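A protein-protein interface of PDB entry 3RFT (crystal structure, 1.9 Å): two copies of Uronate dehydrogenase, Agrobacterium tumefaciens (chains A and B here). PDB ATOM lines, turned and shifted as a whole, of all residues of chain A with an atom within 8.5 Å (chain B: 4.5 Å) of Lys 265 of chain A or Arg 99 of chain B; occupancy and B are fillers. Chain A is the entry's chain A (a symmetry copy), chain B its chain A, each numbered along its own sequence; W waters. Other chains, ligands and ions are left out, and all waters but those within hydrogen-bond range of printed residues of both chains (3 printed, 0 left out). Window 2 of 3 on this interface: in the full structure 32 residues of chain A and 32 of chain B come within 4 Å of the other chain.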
ATOM      1  N   GLU A  77      27.432  11.670  30.840  1.00  0.00           N
ATOM      2  CA  GLU A  77      26.335  10.723  30.649  1.00  0.00           C
ATOM      3  C   GLU A  77      25.069  11.266  31.313  1.00  0.00           C
ATOM      4  O   GLU A  77      25.095  11.673  32.472  1.00  0.00           O
ATOM      5  CB  GLU A  77      26.682   9.341  31.208  1.00  0.00           C
ATOM      6  CG  GLU A  77      25.642   8.262  30.897  1.00  0.00           C
ATOM      7  CD  GLU A  77      25.629   7.843  29.426  1.00  0.00           C
ATOM      8  OE1 GLU A  77      26.450   8.376  28.649  1.00  0.00           O
ATOM      9  OE2 GLU A  77      24.806   6.972  29.054  1.00  0.00           O
ATOM     10  N   LYS A  78      23.970  11.283  30.563  1.00  0.00           N
ATOM     11  CA  LYS A  78      22.700  11.821  31.043  1.00  0.00           C
ATOM     12  C   LYS A  78      21.585  11.037  30.387  1.00  0.00           C
ATOM     13  O   LYS A  78      21.854  10.186  29.543  1.00  0.00           O
ATOM     14  CB  LYS A  78      22.584  13.307  30.692  1.00  0.00           C
ATOM     15  CG  LYS A  78      23.312  14.206  31.678  1.00  0.00           C
ATOM     16  CD  LYS A  78      22.934  15.657  31.499  1.00  0.00           C
ATOM     17  CE  LYS A  78      23.640  16.530  32.523  1.00  0.00           C
ATOM     18  NZ  LYS A  78      23.347  16.101  33.918  1.00  0.00           N
ATOM     19  N   PRO A  79      20.326  11.298  30.776  1.00  0.00           N
ATOM     20  CA  PRO A  79      19.229  10.558  30.148  1.00  0.00           C
ATOM     21  C   PRO A  79      19.109  10.880  28.658  1.00  0.00           C
ATOM     22  O   PRO A  79      19.544  11.946  28.217  1.00  0.00           O
ATOM     23  CB  PRO A  79      17.990  11.055  30.900  1.00  0.00           C
ATOM     24  CG  PRO A  79      18.519  11.459  32.245  1.00  0.00           C
ATOM     25  CD  PRO A  79      19.870  12.066  31.952  1.00  0.00           C
ATOM     26  N   PHE A  80      18.520   9.956  27.910  1.00  0.00           N
ATOM     27  CA  PHE A  80      18.448  10.057  26.449  1.00  0.00           C
ATOM     28  C   PHE A  80      17.811  11.363  25.978  1.00  0.00           C
ATOM     29  O   PHE A  80      18.302  12.003  25.044  1.00  0.00           O
ATOM     30  CB  PHE A  80      17.683   8.861  25.887  1.00  0.00           C
ATOM     31  CG  PHE A  80      17.601   8.845  24.389  1.00  0.00           C
ATOM     32  CD1 PHE A  80      18.721   8.572  23.626  1.00  0.00           C
ATOM     33  CD2 PHE A  80      16.399   9.097  23.745  1.00  0.00           C
ATOM     34  CE1 PHE A  80      18.647   8.554  22.242  1.00  0.00           C
ATOM     35  CE2 PHE A  80      16.320   9.083  22.362  1.00  0.00           C
ATOM     36  CZ  PHE A  80      17.444   8.808  21.614  1.00  0.00           C
ATOM     37  N   GLU A  81      16.720  11.765  26.625  1.00  0.00           N
ATOM     38  CA  GLU A  81      16.016  12.979  26.215  1.00  0.00           C
ATOM     39  C   GLU A  81      16.941  14.194  26.125  1.00  0.00           C
ATOM     40  O   GLU A  81      16.868  14.966  25.167  1.00  0.00           O
ATOM     41  CB  GLU A  81      14.830  13.273  27.140  1.00  0.00           C
ATOM     42  CG  GLU A  81      13.701  12.251  27.049  1.00  0.00           C
ATOM     43  CD  GLU A  81      13.893  11.045  27.968  1.00  0.00           C
ATOM     44  OE1 GLU A  81      15.016  10.841  28.498  1.00  0.00           O
ATOM     45  OE2 GLU A  81      12.906  10.297  28.157  1.00  0.00           O
ATOM     46  N   GLN A  82      17.813  14.366  27.116  1.00  0.00           N
ATOM     47  CA  GLN A  82      18.711  15.518  27.141  1.00  0.00           C
ATOM     48  C   GLN A  82      19.790  15.394  26.065  1.00  0.00           C
ATOM     49  O   GLN A  82      20.137  16.366  25.391  1.00  0.00           O
ATOM     50  CB  GLN A  82      19.379  15.656  28.506  1.00  0.00           C
ATOM     51  CG  GLN A  82      18.410  15.859  29.666  1.00  0.00           C
ATOM     52  CD  GLN A  82      19.144  16.120  30.962  1.00  0.00           C
ATOM     53  OE1 GLN A  82      20.152  16.832  30.984  1.00  0.00           O
ATOM     54  NE2 GLN A  82      18.649  15.543  32.052  1.00  0.00           N
ATOM     55  N   LEU A 135      25.299   6.463  26.386  1.00  0.00           N
ATOM     56  CA  LEU A 135      24.563   7.280  25.414  1.00  0.00           C
ATOM     57  C   LEU A 135      25.328   8.529  25.000  1.00  0.00           C
ATOM     58  O   LEU A 135      25.207   8.990  23.862  1.00  0.00           O
ATOM     59  CB  LEU A 135      23.189   7.676  25.963  1.00  0.00           C
ATOM     60  CG  LEU A 135      22.227   6.530  26.278  1.00  0.00           C
ATOM     61  CD1 LEU A 135      20.995   7.070  27.016  1.00  0.00           C
ATOM     62  CD2 LEU A 135      21.821   5.795  25.018  1.00  0.00           C
ATOM     63  N   PRO A 262      25.000   3.162  34.409  1.00  0.00           N
ATOM     64  CA  PRO A 262      23.809   2.530  33.834  1.00  0.00           C
ATOM     65  C   PRO A 262      23.222   3.470  32.780  1.00  0.00           C
ATOM     66  O   PRO A 262      23.821   4.513  32.506  1.00  0.00           O
ATOM     67  CB  PRO A 262      22.855   2.448  35.026  1.00  0.00           C
ATOM     68  CG  PRO A 262      23.210   3.677  35.855  1.00  0.00           C
ATOM     69  CD  PRO A 262      24.720   3.837  35.694  1.00  0.00           C
ATOM     70  N   ILE A 263      22.072   3.115  32.216  1.00  0.00           N
ATOM     71  CA  ILE A 263      21.301   4.055  31.401  1.00  0.00           C
ATOM     72  C   ILE A 263      20.519   4.935  32.368  1.00  0.00           C
ATOM     73  O   ILE A 263      19.621   4.449  33.060  1.00  0.00           O
ATOM     74  CB  ILE A 263      20.286   3.339  30.500  1.00  0.00           C
ATOM     75  CG1 ILE A 263      20.995   2.344  29.567  1.00  0.00           C
ATOM     76  CG2 ILE A 263      19.465   4.365  29.696  1.00  0.00           C
ATOM     77  CD1 ILE A 263      22.097   2.967  28.743  1.00  0.00           C
ATOM     78  N   PHE A 264      20.888   6.207  32.464  1.00  0.00           N
ATOM     79  CA  PHE A 264      20.206   7.105  33.395  1.00  0.00           C
ATOM     80  C   PHE A 264      18.827   7.473  32.869  1.00  0.00           C
ATOM     81  O   PHE A 264      18.634   7.603  31.660  1.00  0.00           O
ATOM     82  CB  PHE A 264      21.018   8.376  33.617  1.00  0.00           C
ATOM     83  CG  PHE A 264      22.323   8.150  34.324  1.00  0.00           C
ATOM     84  CD1 PHE A 264      22.384   7.368  35.472  1.00  0.00           C
ATOM     85  CD2 PHE A 264      23.484   8.747  33.862  1.00  0.00           C
ATOM     86  CE1 PHE A 264      23.593   7.177  36.133  1.00  0.00           C
ATOM     87  CE2 PHE A 264      24.690   8.562  34.512  1.00  0.00           C
ATOM     88  CZ  PHE A 264      24.745   7.768  35.654  1.00  0.00           C
ATOM     89  N   LYS A 265      17.874   7.649  33.780  1.00  0.00           N
ATOM     90  CA  LYS A 265      16.495   7.936  33.404  1.00  0.00           C
ATOM     91  C   LYS A 265      16.051   9.276  33.978  1.00  0.00           C
ATOM     92  O   LYS A 265      16.526   9.694  35.026  1.00  0.00           O
ATOM     93  CB  LYS A 265      15.574   6.825  33.895  1.00  0.00           C
ATOM     94  CG  LYS A 265      15.938   5.445  33.371  1.00  0.00           C
ATOM     95  CD  LYS A 265      15.470   5.242  31.937  1.00  0.00           C
ATOM     96  CE  LYS A 265      15.742   3.809  31.478  1.00  0.00           C
ATOM     97  NZ  LYS A 265      14.724   3.301  30.507  1.00  0.00           N
ATOM     98  N   GLN A 266      15.138   9.941  33.278  1.00  0.00           N
ATOM     99  CA  GLN A 266      14.745  11.308  33.606  1.00  0.00           C
ATOM    100  C   GLN A 266      13.859  11.393  34.849  1.00  0.00           C
ATOM    101  O   GLN A 266      13.342  10.385  35.330  1.00  0.00           O
ATOM    102  CB  GLN A 266      14.038  11.949  32.406  1.00  0.00           C
ATOM    103  CG  GLN A 266      13.949  13.459  32.481  1.00  0.00           C
ATOM    104  CD  GLN A 266      15.312  14.122  32.445  1.00  0.00           C
ATOM    105  OE1 GLN A 266      15.846  14.525  33.481  1.00  0.00           O
ATOM    106  NE2 GLN A 266      15.883  14.235  31.250  1.00  0.00           N
ATOM    107  N   TYR B  92      16.507   3.596  20.224  1.00  0.00           N
ATOM    108  CA  TYR B  92      16.688   3.671  21.665  1.00  0.00           C
ATOM    109  C   TYR B  92      15.536   2.936  22.367  1.00  0.00           C
ATOM    110  O   TYR B  92      15.758   2.113  23.262  1.00  0.00           O
ATOM    111  CB  TYR B  92      16.799   5.125  22.136  1.00  0.00           C
ATOM    112  CG  TYR B  92      16.717   5.252  23.636  1.00  0.00           C
ATOM    113  CD1 TYR B  92      17.805   4.915  24.444  1.00  0.00           C
ATOM    114  CD2 TYR B  92      15.544   5.679  24.247  1.00  0.00           C
ATOM    115  CE1 TYR B  92      17.723   5.017  25.826  1.00  0.00           C
ATOM    116  CE2 TYR B  92      15.450   5.785  25.624  1.00  0.00           C
ATOM    117  CZ  TYR B  92      16.542   5.447  26.408  1.00  0.00           C
ATOM    118  OH  TYR B  92      16.457   5.553  27.778  1.00  0.00           O
ATOM    119  N   TYR B  95      15.898  -0.900  22.013  1.00  0.00           N
ATOM    120  CA  TYR B  95      16.955  -1.482  22.854  1.00  0.00           C
ATOM    121  C   TYR B  95      16.609  -1.460  24.347  1.00  0.00           C
ATOM    122  O   TYR B  95      16.898  -2.420  25.080  1.00  0.00           O
ATOM    123  CB  TYR B  95      18.350  -0.893  22.540  1.00  0.00           C
ATOM    124  CG  TYR B  95      18.960  -1.675  21.395  1.00  0.00           C
ATOM    125  CD1 TYR B  95      19.888  -2.687  21.629  1.00  0.00           C
ATOM    126  CD2 TYR B  95      18.509  -1.482  20.095  1.00  0.00           C
ATOM    127  CE1 TYR B  95      20.398  -3.454  20.580  1.00  0.00           C
ATOM    128  CE2 TYR B  95      19.006  -2.243  19.037  1.00  0.00           C
ATOM    129  CZ  TYR B  95      19.947  -3.221  19.282  1.00  0.00           C
ATOM    130  OH  TYR B  95      20.422  -3.980  18.239  1.00  0.00           O
ATOM    131  N   GLU B  96      15.970  -0.382  24.788  1.00  0.00           N
ATOM    132  CA  GLU B  96      15.462  -0.325  26.158  1.00  0.00           C
ATOM    133  C   GLU B  96      14.392  -1.389  26.422  1.00  0.00           C
ATOM    134  O   GLU B  96      14.382  -2.030  27.485  1.00  0.00           O
ATOM    135  CB  GLU B  96      14.958   1.085  26.489  1.00  0.00           C
ATOM    136  CG  GLU B  96      16.078   2.016  26.894  1.00  0.00           C
ATOM    137  CD  GLU B  96      16.822   1.492  28.108  1.00  0.00           C
ATOM    138  OE1 GLU B  96      16.233   1.520  29.206  1.00  0.00           O
ATOM    139  OE2 GLU B  96      17.976   1.031  27.969  1.00  0.00           O
ATOM    140  N   ALA B  97      13.503  -1.598  25.456  1.00  0.00           N
ATOM    141  CA  ALA B  97      12.461  -2.610  25.596  1.00  0.00           C
ATOM    142  C   ALA B  97      13.059  -4.013  25.662  1.00  0.00           C
ATOM    143  O   ALA B  97      12.665  -4.830  26.498  1.00  0.00           O
ATOM    144  CB  ALA B  97      11.449  -2.508  24.460  1.00  0.00           C
ATOM    145  N   ALA B  98      14.013  -4.298  24.782  1.00  0.00           N
ATOM    146  CA  ALA B  98      14.721  -5.572  24.842  1.00  0.00           C
ATOM    147  C   ALA B  98      15.412  -5.748  26.203  1.00  0.00           C
ATOM    148  O   ALA B  98      15.349  -6.816  26.805  1.00  0.00           O
ATOM    149  CB  ALA B  98      15.744  -5.684  23.700  1.00  0.00           C
ATOM    150  N   ARG B  99      16.060  -4.693  26.684  1.00  0.00           N
ATOM    151  CA  ARG B  99      16.806  -4.778  27.939  1.00  0.00           C
ATOM    152  C   ARG B  99      15.862  -5.116  29.099  1.00  0.00           C
ATOM    153  O   ARG B  99      16.256  -5.782  30.060  1.00  0.00           O
ATOM    154  CB  ARG B  99      17.567  -3.477  28.218  1.00  0.00           C
ATOM    155  CG  ARG B  99      18.499  -3.550  29.447  1.00  0.00           C
ATOM    156  CD  ARG B  99      19.459  -2.358  29.549  1.00  0.00           C
ATOM    157  NE  ARG B  99      18.779  -1.107  29.886  1.00  0.00           N
ATOM    158  CZ  ARG B  99      18.481  -0.730  31.125  1.00  0.00           C
ATOM    159  NH1 ARG B  99      18.811  -1.505  32.154  1.00  0.00           N
ATOM    160  NH2 ARG B  99      17.857   0.423  31.338  1.00  0.00           N
ATOM    161  N   ALA B 100      14.614  -4.671  28.990  1.00  0.00           N
ATOM    162  CA  ALA B 100      13.633  -4.876  30.057  1.00  0.00           C
ATOM    163  C   ALA B 100      12.915  -6.220  29.959  1.00  0.00           C
ATOM    164  O   ALA B 100      12.198  -6.618  30.885  1.00  0.00           O
ATOM    165  CB  ALA B 100      12.624  -3.727  30.081  1.00  0.00           C
ATOM    166  N   HIS B 101      13.118  -6.925  28.850  1.00  0.00           N
ATOM    167  CA  HIS B 101      12.389  -8.161  28.588  1.00  0.00           C
ATOM    168  C   HIS B 101      13.255  -9.343  28.166  1.00  0.00           C
ATOM    169  O   HIS B 101      12.896 -10.096  27.261  1.00  0.00           O
ATOM    170  CB  HIS B 101      11.252  -7.912  27.587  1.00  0.00           C
ATOM    171  CG  HIS B 101      10.189  -7.005  28.119  1.00  0.00           C
ATOM    172  ND1 HIS B 101       9.257  -7.420  29.048  1.00  0.00           N
ATOM    173  CD2 HIS B 101       9.934  -5.696  27.889  1.00  0.00           C
ATOM    174  CE1 HIS B 101       8.463  -6.408  29.352  1.00  0.00           C
ATOM    175  NE2 HIS B 101       8.853  -5.351  28.664  1.00  0.00           N
ATOM    176  N   GLY B 102      14.385  -9.520  28.844  1.00  0.00           N
ATOM    177  CA  GLY B 102      15.183 -10.720  28.673  1.00  0.00           C
ATOM    178  C   GLY B 102      16.242 -10.659  27.582  1.00  0.00           C
ATOM    179  O   GLY B 102      16.871 -11.666  27.279  1.00  0.00           O
ATOM    180  N   GLN B 103      16.444  -9.476  27.005  1.00  0.00           N
ATOM    181  CA  GLN B 103      17.422  -9.284  25.930  1.00  0.00           C
ATOM    182  C   GLN B 103      17.318 -10.286  24.771  1.00  0.00           C
ATOM    183  O   GLN B 103      18.300 -10.925  24.405  1.00  0.00           O
ATOM    184  CB  GLN B 103      18.848  -9.220  26.508  1.00  0.00           C
ATOM    185  CG  GLN B 103      18.990  -8.049  27.462  1.00  0.00           C
ATOM    186  CD  GLN B 103      20.368  -7.872  28.074  1.00  0.00           C
ATOM    187  OE1 GLN B 103      20.599  -6.894  28.785  1.00  0.00           O
ATOM    188  NE2 GLN B 103      21.282  -8.796  27.804  1.00  0.00           N
ATOM    189  N   TYR B 150      25.132  -1.369  23.926  1.00  0.00           N
ATOM    190  CA  TYR B 150      24.318  -2.304  24.713  1.00  0.00           C
ATOM    191  C   TYR B 150      24.975  -3.676  24.823  1.00  0.00           C
ATOM    192  O   TYR B 150      24.795  -4.377  25.826  1.00  0.00           O
ATOM    193  CB  TYR B 150      22.893  -2.438  24.144  1.00  0.00           C
ATOM    194  CG  TYR B 150      21.980  -1.333  24.629  1.00  0.00           C
ATOM    195  CD1 TYR B 150      21.049  -1.561  25.636  1.00  0.00           C
ATOM    196  CD2 TYR B 150      22.073  -0.048  24.100  1.00  0.00           C
ATOM    197  CE1 TYR B 150      20.219  -0.537  26.094  1.00  0.00           C
ATOM    198  CE2 TYR B 150      21.249   0.981  24.547  1.00  0.00           C
ATOM    199  CZ  TYR B 150      20.329   0.731  25.548  1.00  0.00           C
ATOM    200  OH  TYR B 150      19.513   1.755  25.989  1.00  0.00           O
ATOM    201  N   PHE B 154      25.716  -4.501  28.520  1.00  0.00           N
ATOM    202  CA  PHE B 154      24.694  -5.401  29.050  1.00  0.00           C
ATOM    203  C   PHE B 154      24.729  -6.809  28.461  1.00  0.00           C
ATOM    204  O   PHE B 154      24.036  -7.703  28.949  1.00  0.00           O
ATOM    205  CB  PHE B 154      23.298  -4.810  28.823  1.00  0.00           C
ATOM    206  CG  PHE B 154      23.099  -3.476  29.467  1.00  0.00           C
ATOM    207  CD1 PHE B 154      23.018  -3.370  30.850  1.00  0.00           C
ATOM    208  CD2 PHE B 154      22.985  -2.327  28.697  1.00  0.00           C
ATOM    209  CE1 PHE B 154      22.831  -2.144  31.446  1.00  0.00           C
ATOM    210  CE2 PHE B 154      22.796  -1.098  29.289  1.00  0.00           C
ATOM    211  CZ  PHE B 154      22.721  -1.001  30.665  1.00  0.00           C
HETATM  212  O   HOH W   1      20.925   0.641  33.285  1.00  0.00           O
HETATM  213  O   HOH W   2      13.929   5.604  28.803  1.00  0.00           O
HETATM  214  O   HOH W   3      17.559   7.524  29.165  1.00  0.00           O
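The side-chain amino group of Lys 265 of chain A is in salt-bridge range of the side-chain carboxylate of Glu 96 of chain B.
The side-chain carboxylate (OE2) of Glu 96 of chain B sits at hydrogen-bond distance from the side-chain hydroxyl (OH) of Tyr 150 of chain B (2.6 Å). The side-chain amide nitrogen (NE2) of Gln 103 of chain B lies within hydrogen-bond range of the backbone carbonyl oxygen (O) of Phe 154 of chain B, at 3.2 Å. OE1 of Glu 96 of chain B lies within salt-bridge range of NH2 of Arg 99 of chain B.
Tyr 92 of chain B touches Phe 80 of chain A (CD2 to CD2, 3.6 Å). Ile 263 of chain A touches Tyr 92 of chain B. Glu 96 of chain B touches Ile 263 of chain A. Ile 263 of chain A touches Arg 99 of chain B. Ile 263 of chain A touches Tyr 150 of chain B. Ile 263 of chain A touches Phe 154 of chain B (CG1 to CE2, 3.9 Å). Lys 265 of chain A touches Tyr 92 of chain B. Lys 265 of chain A touches Arg 99 of chain B.
Water W3 lies within hydrogen-bond range of OH of Tyr 92 of chain B, O of Phe 264 of chain A and N of Phe 80 of chain A. Water W2 bridges the side-chain hydroxyl of Tyr 92 of chain B (2.7 Å) and the side-chain amino group of Lys 265 of chain A (3.0 Å). Water W1 bridges N of Ile 263 of chain A (2.9 Å) and NH1 of Arg 99 of chain B (3.2 Å).
No position is printed for both chains. Of the 9 pairs that touch across the chains among the printed residues, none has its exchanged pair printed and touching as well.
Of the printed residues of chain B, Lys 265 of chain A touches Tyr 92, Glu 96 and Arg 99. Of the printed residues of chain A, Arg 99 of chain B touches Ile 263 and Lys 265. No residue of chain A comes within 4 Å of Ala 100 of chain B. Of the printed residues of chain A, Phe 154 of chain B touches Ile 263. Printed residues of chain B within 4 Å of Ile 263 of chain A: Tyr 92 (3.8 Å), Glu 96 (3.7 Å), Arg 99 (3.9 Å), Tyr 150 (3.9 Å) and Phe 154 (3.9 Å). Of the printed residues of chain A, Tyr 150 of chain B touches Ile 263 (3.9 Å). Gln 82 of chain A touches none of the printed residues of chain B. The nearest printed residue of chain A that does not touch Arg 99 of chain B is Pro 262 of chain A (6.3 Å).
Hydrophobic or aromatic side chains of chain A within 4 Å of the printed part of chain B: Phe 80 and Ile 263. Of the 12 printed residues of chain B, 5 touch a printed residue of chain A. Hydrophobic or aromatic side chains of chain B within 4 Å of the printed part of chain A: Tyr 92, Tyr 150 and Phe 154. Among the printed residues, Asp or Glu carboxylates within 4 Å of a Lys or Arg side-chain nitrogen of the other chain: Lys 265 of chain A with Glu 96 of chain B (2.7 Å).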
